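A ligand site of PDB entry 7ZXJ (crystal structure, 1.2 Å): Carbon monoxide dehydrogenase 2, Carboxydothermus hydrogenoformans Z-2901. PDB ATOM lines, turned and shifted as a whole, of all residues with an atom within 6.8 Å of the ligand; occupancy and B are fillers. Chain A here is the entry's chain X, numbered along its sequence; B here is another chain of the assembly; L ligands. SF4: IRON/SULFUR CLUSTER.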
ATOM      1  N   CYS A  47     -19.572  20.567 -14.226  1.00  0.00           N
ATOM      2  CA  CYS A  47     -20.616  21.330 -13.545  1.00  0.00           C
ATOM      3  C   CYS A  47     -20.244  21.378 -12.074  1.00  0.00           C
ATOM      4  O   CYS A  47     -19.783  20.377 -11.504  1.00  0.00           O
ATOM      5  CB  CYS A  47     -21.977  20.686 -13.696  1.00  0.00           C
ATOM      6  SG  CYS A  47     -23.275  21.599 -12.831  1.00  0.00           S
ATOM      7  N   CYS A  48     -20.477  22.528 -11.443  1.00  0.00           N
ATOM      8  CA  CYS A  48     -20.226  22.716 -10.023  1.00  0.00           C
ATOM      9  C   CYS A  48     -21.375  23.480  -9.403  1.00  0.00           C
ATOM     10  O   CYS A  48     -21.801  24.517  -9.930  1.00  0.00           O
ATOM     11  CB  CYS A  48     -18.926  23.489  -9.783  1.00  0.00           C
ATOM     12  SG  CYS A  48     -18.515  23.741  -8.054  1.00  0.00           S
ATOM     13  N   ARG A  49     -21.848  22.983  -8.261  1.00  0.00           N
ATOM     14  CA  ARG A  49     -22.880  23.627  -7.469  1.00  0.00           C
ATOM     15  C   ARG A  49     -22.407  23.757  -6.032  1.00  0.00           C
ATOM     16  O   ARG A  49     -23.211  23.733  -5.095  1.00  0.00           O
ATOM     17  CB  ARG A  49     -24.174  22.838  -7.571  1.00  0.00           C
ATOM     18  CG  ARG A  49     -24.740  22.811  -8.971  1.00  0.00           C
ATOM     19  CD  ARG A  49     -25.887  21.814  -9.066  1.00  0.00           C
ATOM     20  NE  ARG A  49     -26.941  22.152  -8.133  1.00  0.00           N
ATOM     21  CZ  ARG A  49     -27.878  21.331  -7.699  1.00  0.00           C
ATOM     22  NH1 ARG A  49     -27.916  20.072  -8.125  1.00  0.00           N
ATOM     23  NH2 ARG A  49     -28.774  21.765  -6.828  1.00  0.00           N
ATOM     24  N   HIS A  50     -21.098  23.928  -5.820  1.00  0.00           N
ATOM     25  CA  HIS A  50     -20.546  23.980  -4.474  1.00  0.00           C
ATOM     26  C   HIS A  50     -20.735  25.324  -3.783  1.00  0.00           C
ATOM     27  O   HIS A  50     -20.372  25.441  -2.611  1.00  0.00           O
ATOM     28  CB  HIS A  50     -19.078  23.512  -4.442  1.00  0.00           C
ATOM     29  CG  HIS A  50     -18.903  22.067  -4.779  1.00  0.00           C
ATOM     30  ND1 HIS A  50     -17.739  21.370  -4.515  1.00  0.00           N
ATOM     31  CD2 HIS A  50     -19.728  21.191  -5.398  1.00  0.00           C
ATOM     32  CE1 HIS A  50     -17.874  20.120  -4.934  1.00  0.00           C
ATOM     33  NE2 HIS A  50     -19.069  19.984  -5.472  1.00  0.00           N
ATOM     34  N   CYS A  51     -21.279  26.331  -4.454  1.00  0.00           N
ATOM     35  CA  CYS A  51     -21.685  27.538  -3.725  1.00  0.00           C
ATOM     36  C   CYS A  51     -22.882  28.170  -4.427  1.00  0.00           C
ATOM     37  O   CYS A  51     -23.299  27.735  -5.506  1.00  0.00           O
ATOM     38  CB  CYS A  51     -20.537  28.535  -3.540  1.00  0.00           C
ATOM     39  SG  CYS A  51     -20.184  29.594  -4.972  1.00  0.00           S
ATOM     40  N   LEU A  52     -23.452  29.186  -3.778  1.00  0.00           N
ATOM     41  CA  LEU A  52     -24.652  29.855  -4.252  1.00  0.00           C
ATOM     42  C   LEU A  52     -24.379  30.875  -5.351  1.00  0.00           C
ATOM     43  O   LEU A  52     -25.308  31.550  -5.827  1.00  0.00           O
ATOM     44  CB  LEU A  52     -25.435  30.480  -3.090  1.00  0.00           C
ATOM     45  CG  LEU A  52     -25.874  29.494  -2.027  1.00  0.00           C
ATOM     46  CD1 LEU A  52     -26.569  30.226  -0.931  1.00  0.00           C
ATOM     47  CD2 LEU A  52     -26.802  28.427  -2.616  1.00  0.00           C
ATOM     48  N   GLN A  53     -23.132  30.989  -5.799  1.00  0.00           N
ATOM     49  CA  GLN A  53     -22.865  31.706  -7.044  1.00  0.00           C
ATOM     50  C   GLN A  53     -23.129  30.832  -8.254  1.00  0.00           C
ATOM     51  O   GLN A  53     -23.314  31.362  -9.353  1.00  0.00           O
ATOM     52  CB  GLN A  53     -21.436  32.251  -7.078  1.00  0.00           C
ATOM     53  CG  GLN A  53     -21.208  33.306  -6.051  1.00  0.00           C
ATOM     54  CD  GLN A  53     -19.811  33.868  -6.067  1.00  0.00           C
ATOM     55  OE1 GLN A  53     -18.845  33.204  -6.423  1.00  0.00           O
ATOM     56  NE2 GLN A  53     -19.697  35.096  -5.669  1.00  0.00           N
ATOM     57  N   GLY A  54     -23.150  29.506  -8.068  1.00  0.00           N
ATOM     58  CA  GLY A  54     -23.461  28.625  -9.161  1.00  0.00           C
ATOM     59  C   GLY A  54     -24.941  28.573  -9.468  1.00  0.00           C
ATOM     60  O   GLY A  54     -25.745  29.338  -8.914  1.00  0.00           O
ATOM     61  N   PRO A  55     -25.338  27.655 -10.348  1.00  0.00           N
ATOM     62  CA  PRO A  55     -24.479  26.603 -10.897  1.00  0.00           C
ATOM     63  C   PRO A  55     -23.494  27.143 -11.909  1.00  0.00           C
ATOM     64  O   PRO A  55     -23.793  28.066 -12.715  1.00  0.00           O
ATOM     65  CB  PRO A  55     -25.484  25.663 -11.569  1.00  0.00           C
ATOM     66  CG  PRO A  55     -26.666  26.569 -11.879  1.00  0.00           C
ATOM     67  CD  PRO A  55     -26.729  27.543 -10.778  1.00  0.00           C
ATOM     68  N   CYS A  56     -22.288  26.593 -11.847  1.00  0.00           N
ATOM     69  CA  CYS A  56     -21.255  26.838 -12.854  1.00  0.00           C
ATOM     70  C   CYS A  56     -21.074  25.620 -13.747  1.00  0.00           C
ATOM     71  O   CYS A  56     -21.226  24.481 -13.299  1.00  0.00           O
ATOM     72  CB  CYS A  56     -19.917  27.187 -12.187  1.00  0.00           C
ATOM     73  SG  CYS A  56     -19.948  28.799 -11.353  1.00  0.00           S
ATOM     74  N   ARG A  57     -20.720  25.882 -15.001  1.00  0.00           N
ATOM     75  CA  ARG A  57     -20.395  24.843 -15.957  1.00  0.00           C
ATOM     76  C   ARG A  57     -19.254  25.335 -16.820  1.00  0.00           C
ATOM     77  O   ARG A  57     -18.960  26.529 -16.887  1.00  0.00           O
ATOM     78  CB  ARG A  57     -21.596  24.481 -16.851  1.00  0.00           C
ATOM     79  CG  ARG A  57     -21.957  25.596 -17.827  1.00  0.00           C
ATOM     80  CD  ARG A  57     -23.383  25.555 -18.355  1.00  0.00           C
ATOM     81  NE  ARG A  57     -23.543  26.616 -19.349  1.00  0.00           N
ATOM     82  CZ  ARG A  57     -23.708  27.897 -19.060  1.00  0.00           C
ATOM     83  NH1 ARG A  57     -23.753  28.781 -20.048  1.00  0.00           N
ATOM     84  NH2 ARG A  57     -23.857  28.324 -17.797  1.00  0.00           N
ATOM     85  N   VAL A  67     -14.256  28.589 -17.334  1.00  0.00           N
ATOM     86  CA  VAL A  67     -13.750  28.547 -15.969  1.00  0.00           C
ATOM     87  C   VAL A  67     -14.925  28.875 -15.059  1.00  0.00           C
ATOM     88  O   VAL A  67     -15.843  29.611 -15.429  1.00  0.00           O
ATOM     89  CB  VAL A  67     -12.543  29.516 -15.816  1.00  0.00           C
ATOM     90  CG1 VAL A  67     -12.966  30.928 -16.148  1.00  0.00           C
ATOM     91  CG2 VAL A  67     -11.956  29.454 -14.444  1.00  0.00           C
ATOM     92  N   GLY A  68     -14.911  28.317 -13.858  1.00  0.00           N
ATOM     93  CA  GLY A  68     -15.928  28.648 -12.885  1.00  0.00           C
ATOM     94  C   GLY A  68     -15.849  30.091 -12.411  1.00  0.00           C
ATOM     95  O   GLY A  68     -14.849  30.778 -12.556  1.00  0.00           O
ATOM     96  N   ILE A  69     -16.948  30.545 -11.804  1.00  0.00           N
ATOM     97  CA  ILE A  69     -17.059  31.958 -11.401  1.00  0.00           C
ATOM     98  C   ILE A  69     -15.959  32.349 -10.424  1.00  0.00           C
ATOM     99  O   ILE A  69     -15.373  33.430 -10.543  1.00  0.00           O
ATOM    100  CB  ILE A  69     -18.468  32.289 -10.884  1.00  0.00           C
ATOM    101  CG1 ILE A  69     -19.476  32.247 -12.049  1.00  0.00           C
ATOM    102  CG2 ILE A  69     -18.503  33.626 -10.143  1.00  0.00           C
ATOM    103  CD1 ILE A  69     -20.911  32.382 -11.588  1.00  0.00           C
ATOM    104  N   CYS A  70     -15.650  31.490  -9.453  1.00  0.00           N
ATOM    105  CA  CYS A  70     -14.565  31.742  -8.506  1.00  0.00           C
ATOM    106  C   CYS A  70     -13.161  31.538  -9.091  1.00  0.00           C
ATOM    107  O   CYS A  70     -12.175  31.794  -8.374  1.00  0.00           O
ATOM    108  CB  CYS A  70     -14.716  30.803  -7.326  1.00  0.00           C
ATOM    109  SG  CYS A  70     -14.589  29.084  -7.772  1.00  0.00           S
ATOM    110  N   GLY A  71     -13.053  31.081 -10.348  1.00  0.00           N
ATOM    111  CA  GLY A  71     -11.780  30.752 -10.947  1.00  0.00           C
ATOM    112  C   GLY A  71     -11.461  29.263 -10.961  1.00  0.00           C
ATOM    113  O   GLY A  71     -10.400  28.877 -11.429  1.00  0.00           O
ATOM    114  N   ALA A  72     -12.379  28.410 -10.500  1.00  0.00           N
ATOM    115  CA  ALA A  72     -12.127  26.986 -10.477  1.00  0.00           C
ATOM    116  C   ALA A  72     -12.005  26.457 -11.900  1.00  0.00           C
ATOM    117  O   ALA A  72     -12.901  26.649 -12.724  1.00  0.00           O
ATOM    118  CB  ALA A  72     -13.284  26.298  -9.764  1.00  0.00           C
ATOM    119  N   ILE A  77     -12.788  21.400 -10.755  1.00  0.00           N
ATOM    120  CA  ILE A  77     -14.195  21.027 -10.682  1.00  0.00           C
ATOM    121  C   ILE A  77     -14.346  19.513 -10.792  1.00  0.00           C
ATOM    122  O   ILE A  77     -15.056  18.885  -9.997  1.00  0.00           O
ATOM    123  CB  ILE A  77     -15.006  21.794 -11.748  1.00  0.00           C
ATOM    124  CG1 ILE A  77     -15.135  23.253 -11.322  1.00  0.00           C
ATOM    125  CG2 ILE A  77     -16.372  21.153 -11.974  1.00  0.00           C
ATOM    126  CD1 ILE A  77     -15.705  24.176 -12.395  1.00  0.00           C
ATOM    127  N   ARG A  80     -12.974  17.751  -7.592  1.00  0.00           N
ATOM    128  CA  ARG A  80     -13.808  17.984  -6.409  1.00  0.00           C
ATOM    129  C   ARG A  80     -15.072  17.141  -6.462  1.00  0.00           C
ATOM    130  O   ARG A  80     -15.475  16.546  -5.438  1.00  0.00           O
ATOM    131  CB  ARG A  80     -14.160  19.467  -6.260  1.00  0.00           C
ATOM    132  CG  ARG A  80     -12.949  20.353  -5.946  1.00  0.00           C
ATOM    133  CD  ARG A  80     -13.309  21.770  -5.523  1.00  0.00           C
ATOM    134  NE  ARG A  80     -14.181  22.445  -6.484  1.00  0.00           N
ATOM    135  CZ  ARG A  80     -14.434  23.749  -6.435  1.00  0.00           C
ATOM    136  NH1 ARG A  80     -13.832  24.500  -5.523  1.00  0.00           N
ATOM    137  NH2 ARG A  80     -15.249  24.332  -7.303  1.00  0.00           N
ATOM    138  N   THR A 197     -13.142  20.235  -0.626  1.00  0.00           N
ATOM    139  CA  THR A 197     -13.865  20.417  -1.870  1.00  0.00           C
ATOM    140  C   THR A 197     -14.871  21.566  -1.828  1.00  0.00           C
ATOM    141  O   THR A 197     -15.465  21.879  -2.874  1.00  0.00           O
ATOM    142  CB  THR A 197     -14.581  19.140  -2.297  1.00  0.00           C
ATOM    143  OG1 THR A 197     -15.488  18.734  -1.270  1.00  0.00           O
ATOM    144  CG2 THR A 197     -13.575  18.011  -2.603  1.00  0.00           C
ATOM    145  N   SER A 198     -15.080  22.170  -0.671  1.00  0.00           N
ATOM    146  CA  SER A 198     -15.961  23.326  -0.574  1.00  0.00           C
ATOM    147  C   SER A 198     -15.294  24.536  -1.232  1.00  0.00           C
ATOM    148  O   SER A 198     -14.112  24.535  -1.571  1.00  0.00           O
ATOM    149  CB  SER A 198     -16.387  23.580   0.885  1.00  0.00           C
ATOM    150  OG  SER A 198     -15.369  24.153   1.675  1.00  0.00           O
ATOM    151  N   MET A 199     -16.093  25.577  -1.476  1.00  0.00           N
ATOM    152  CA  MET A 199     -15.606  26.705  -2.273  1.00  0.00           C
ATOM    153  C   MET A 199     -14.393  27.351  -1.613  1.00  0.00           C
ATOM    154  O   MET A 199     -14.332  27.550  -0.385  1.00  0.00           O
ATOM    155  CB  MET A 199     -16.739  27.719  -2.486  1.00  0.00           C
ATOM    156  CG  MET A 199     -16.329  28.947  -3.308  1.00  0.00           C
ATOM    157  SD  MET A 199     -15.524  30.213  -2.265  1.00  0.00           S
ATOM    158  CE  MET A 199     -14.614  31.120  -3.505  1.00  0.00           C
ATOM    159  N   GLY A 200     -13.397  27.651  -2.440  1.00  0.00           N
ATOM    160  CA  GLY A 200     -12.274  28.460  -1.994  1.00  0.00           C
ATOM    161  C   GLY A 200     -11.277  27.718  -1.139  1.00  0.00           C
ATOM    162  O   GLY A 200     -10.539  28.336  -0.360  1.00  0.00           O
ATOM    163  N   MET B  35     -20.766  33.172 -17.662  1.00  0.00           N
ATOM    164  CA  MET B  35     -21.544  32.019 -17.234  1.00  0.00           C
ATOM    165  C   MET B  35     -23.025  32.162 -17.542  1.00  0.00           C
ATOM    166  O   MET B  35     -23.776  31.181 -17.437  1.00  0.00           O
ATOM    167  CB  MET B  35     -21.362  31.808 -15.721  1.00  0.00           C
ATOM    168  CG  MET B  35     -21.713  30.389 -15.258  1.00  0.00           C
ATOM    169  SD  MET B  35     -20.696  29.112 -16.002  1.00  0.00           S
ATOM    170  CE  MET B  35     -19.124  29.451 -15.193  1.00  0.00           C
ATOM    171  N   GLN B  38     -27.262  31.042 -16.494  1.00  0.00           N
ATOM    172  CA  GLN B  38     -26.941  29.863 -15.705  1.00  0.00           C
ATOM    173  C   GLN B  38     -28.035  28.817 -15.815  1.00  0.00           C
ATOM    174  O   GLN B  38     -29.176  29.104 -16.150  1.00  0.00           O
ATOM    175  CB  GLN B  38     -26.705  30.261 -14.241  1.00  0.00           C
ATOM    176  CG  GLN B  38     -25.455  31.106 -14.080  1.00  0.00           C
ATOM    177  CD  GLN B  38     -25.179  31.548 -12.662  1.00  0.00           C
ATOM    178  OE1 GLN B  38     -25.755  32.522 -12.182  1.00  0.00           O
ATOM    179  NE2 GLN B  38     -24.310  30.838 -11.982  1.00  0.00           N
ATOM    180  N   PRO B 336      -9.717  30.760  -6.387  1.00  0.00           N
ATOM    181  CA  PRO B 336      -8.445  30.241  -6.904  1.00  0.00           C
ATOM    182  C   PRO B 336      -7.882  31.053  -8.063  1.00  0.00           C
ATOM    183  O   PRO B 336      -6.691  30.905  -8.388  1.00  0.00           O
ATOM    184  CB  PRO B 336      -8.764  28.782  -7.278  1.00  0.00           C
ATOM    185  CG  PRO B 336     -10.242  28.784  -7.523  1.00  0.00           C
ATOM    186  CD  PRO B 336     -10.814  29.770  -6.533  1.00  0.00           C
ATOM    187  N   MET B 560     -23.202  33.043   0.035  1.00  0.00           N
ATOM    188  CA  MET B 560     -22.489  32.349  -1.044  1.00  0.00           C
ATOM    189  C   MET B 560     -22.040  30.942  -0.641  1.00  0.00           C
ATOM    190  O   MET B 560     -22.409  29.950  -1.276  1.00  0.00           O
ATOM    191  CB  MET B 560     -21.301  33.208  -1.508  1.00  0.00           C
ATOM    192  CG  MET B 560     -20.405  32.589  -2.565  1.00  0.00           C
ATOM    193  SD  MET B 560     -19.015  31.591  -1.973  1.00  0.00           S
ATOM    194  CE  MET B 560     -18.054  32.772  -1.077  1.00  0.00           C
HETATM  195 FE1  SF4 L   1     -19.060  28.208  -9.288  1.00  0.00          FE
HETATM  196 FE2  SF4 L   1     -19.210  28.277  -6.569  1.00  0.00          FE
HETATM  197 FE3  SF4 L   1     -18.421  26.044  -7.866  1.00  0.00          FE
HETATM  198 FE4  SF4 L   1     -16.719  28.167  -7.839  1.00  0.00          FE
HETATM  199  S1  SF4 L   1     -17.437  26.885  -6.070  1.00  0.00           S
HETATM  200  S2  SF4 L   1     -17.193  26.882  -9.615  1.00  0.00           S
HETATM  201  S3  SF4 L   1     -18.297  29.853  -7.964  1.00  0.00           S
HETATM  202  S4  SF4 L   1     -20.449  27.002  -7.918  1.00  0.00           S
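Gly 68 touches the ligand. Ile 69 touches the ligand (CB to S3, 3.8 Å). Ala 72 touches the ligand (CB to S2, 3.96 Å). Met 199 touches the ligand. Hydrophobic or aromatic side chains within 4 Å of the ligand: Ile 69, Ala 72 and Met 199. 12 residues have an atom within 4 Å of the ligand: Cys 48, His 50, Cys 51, Gln 53, Gly 54, Cys 56, Gly 68, Ile 69, Cys 70, Ala 72, Arg 80 and Met 199.
S4 of the ligand lies close to N of Cys 51, 3.6 Å away. The side-chain sulfur (SG) of Cys 51 binds an iron atom (FE2) of the ligand, at 2.3 Å. The side-chain sulfur (SG) of Cys 48 is bound to an iron atom (FE3) of the ligand (2.3 Å). N of Cys 70 lies close to S3 of the ligand, at 3.5 Å. FE4 of the ligand is bound by SG of Cys 70 (2.3 Å). FE1 of the ligand is bound by SG of Cys 56, at 2.3 Å. A sulfur (S1) of the ligand sits close to the guanidinium group (NH2) of Arg 80 (3.6 Å). The backbone NH of Gly 54 sits close to a sulfur (S4) of the ligand, at 3.7 Å. S3 of the ligand lies close to OE1 of Gln 53 (3.7 Å). The backbone NH (N) of His 50 sits close to a sulfur (S4) of the ligand (3.8 Å).
The side-chain sulfur (SG) of Cys 51 sits close to the side-chain sulfur (SD) of Met 560 of chain B, 3.8 Å away. The backbone carbonyl oxygen (O) of Cys 56 lies within hydrogen-bond range of the backbone NH (N) of Cys 48 (2.8 Å). SG of Cys 48 lies close to NH2 of Arg 80, 3.4 Å away. SG of Cys 48 sits close to N of His 50. The side-chain sulfur (SG) of Cys 56 lies close to the backbone NH (N) of Ile 69. The backbone carbonyl oxygen (O) of Cys 56 sits close to the side-chain sulfur (SG) of Cys 47, at 3.6 Å. The backbone carbonyl oxygen (O) of Gln 53 sits at hydrogen-bond distance from the side-chain amide nitrogen (NE2) of Gln 38 of chain B. ND1 of His 50 sits at hydrogen-bond distance from O of Thr 197 (2.9 Å).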
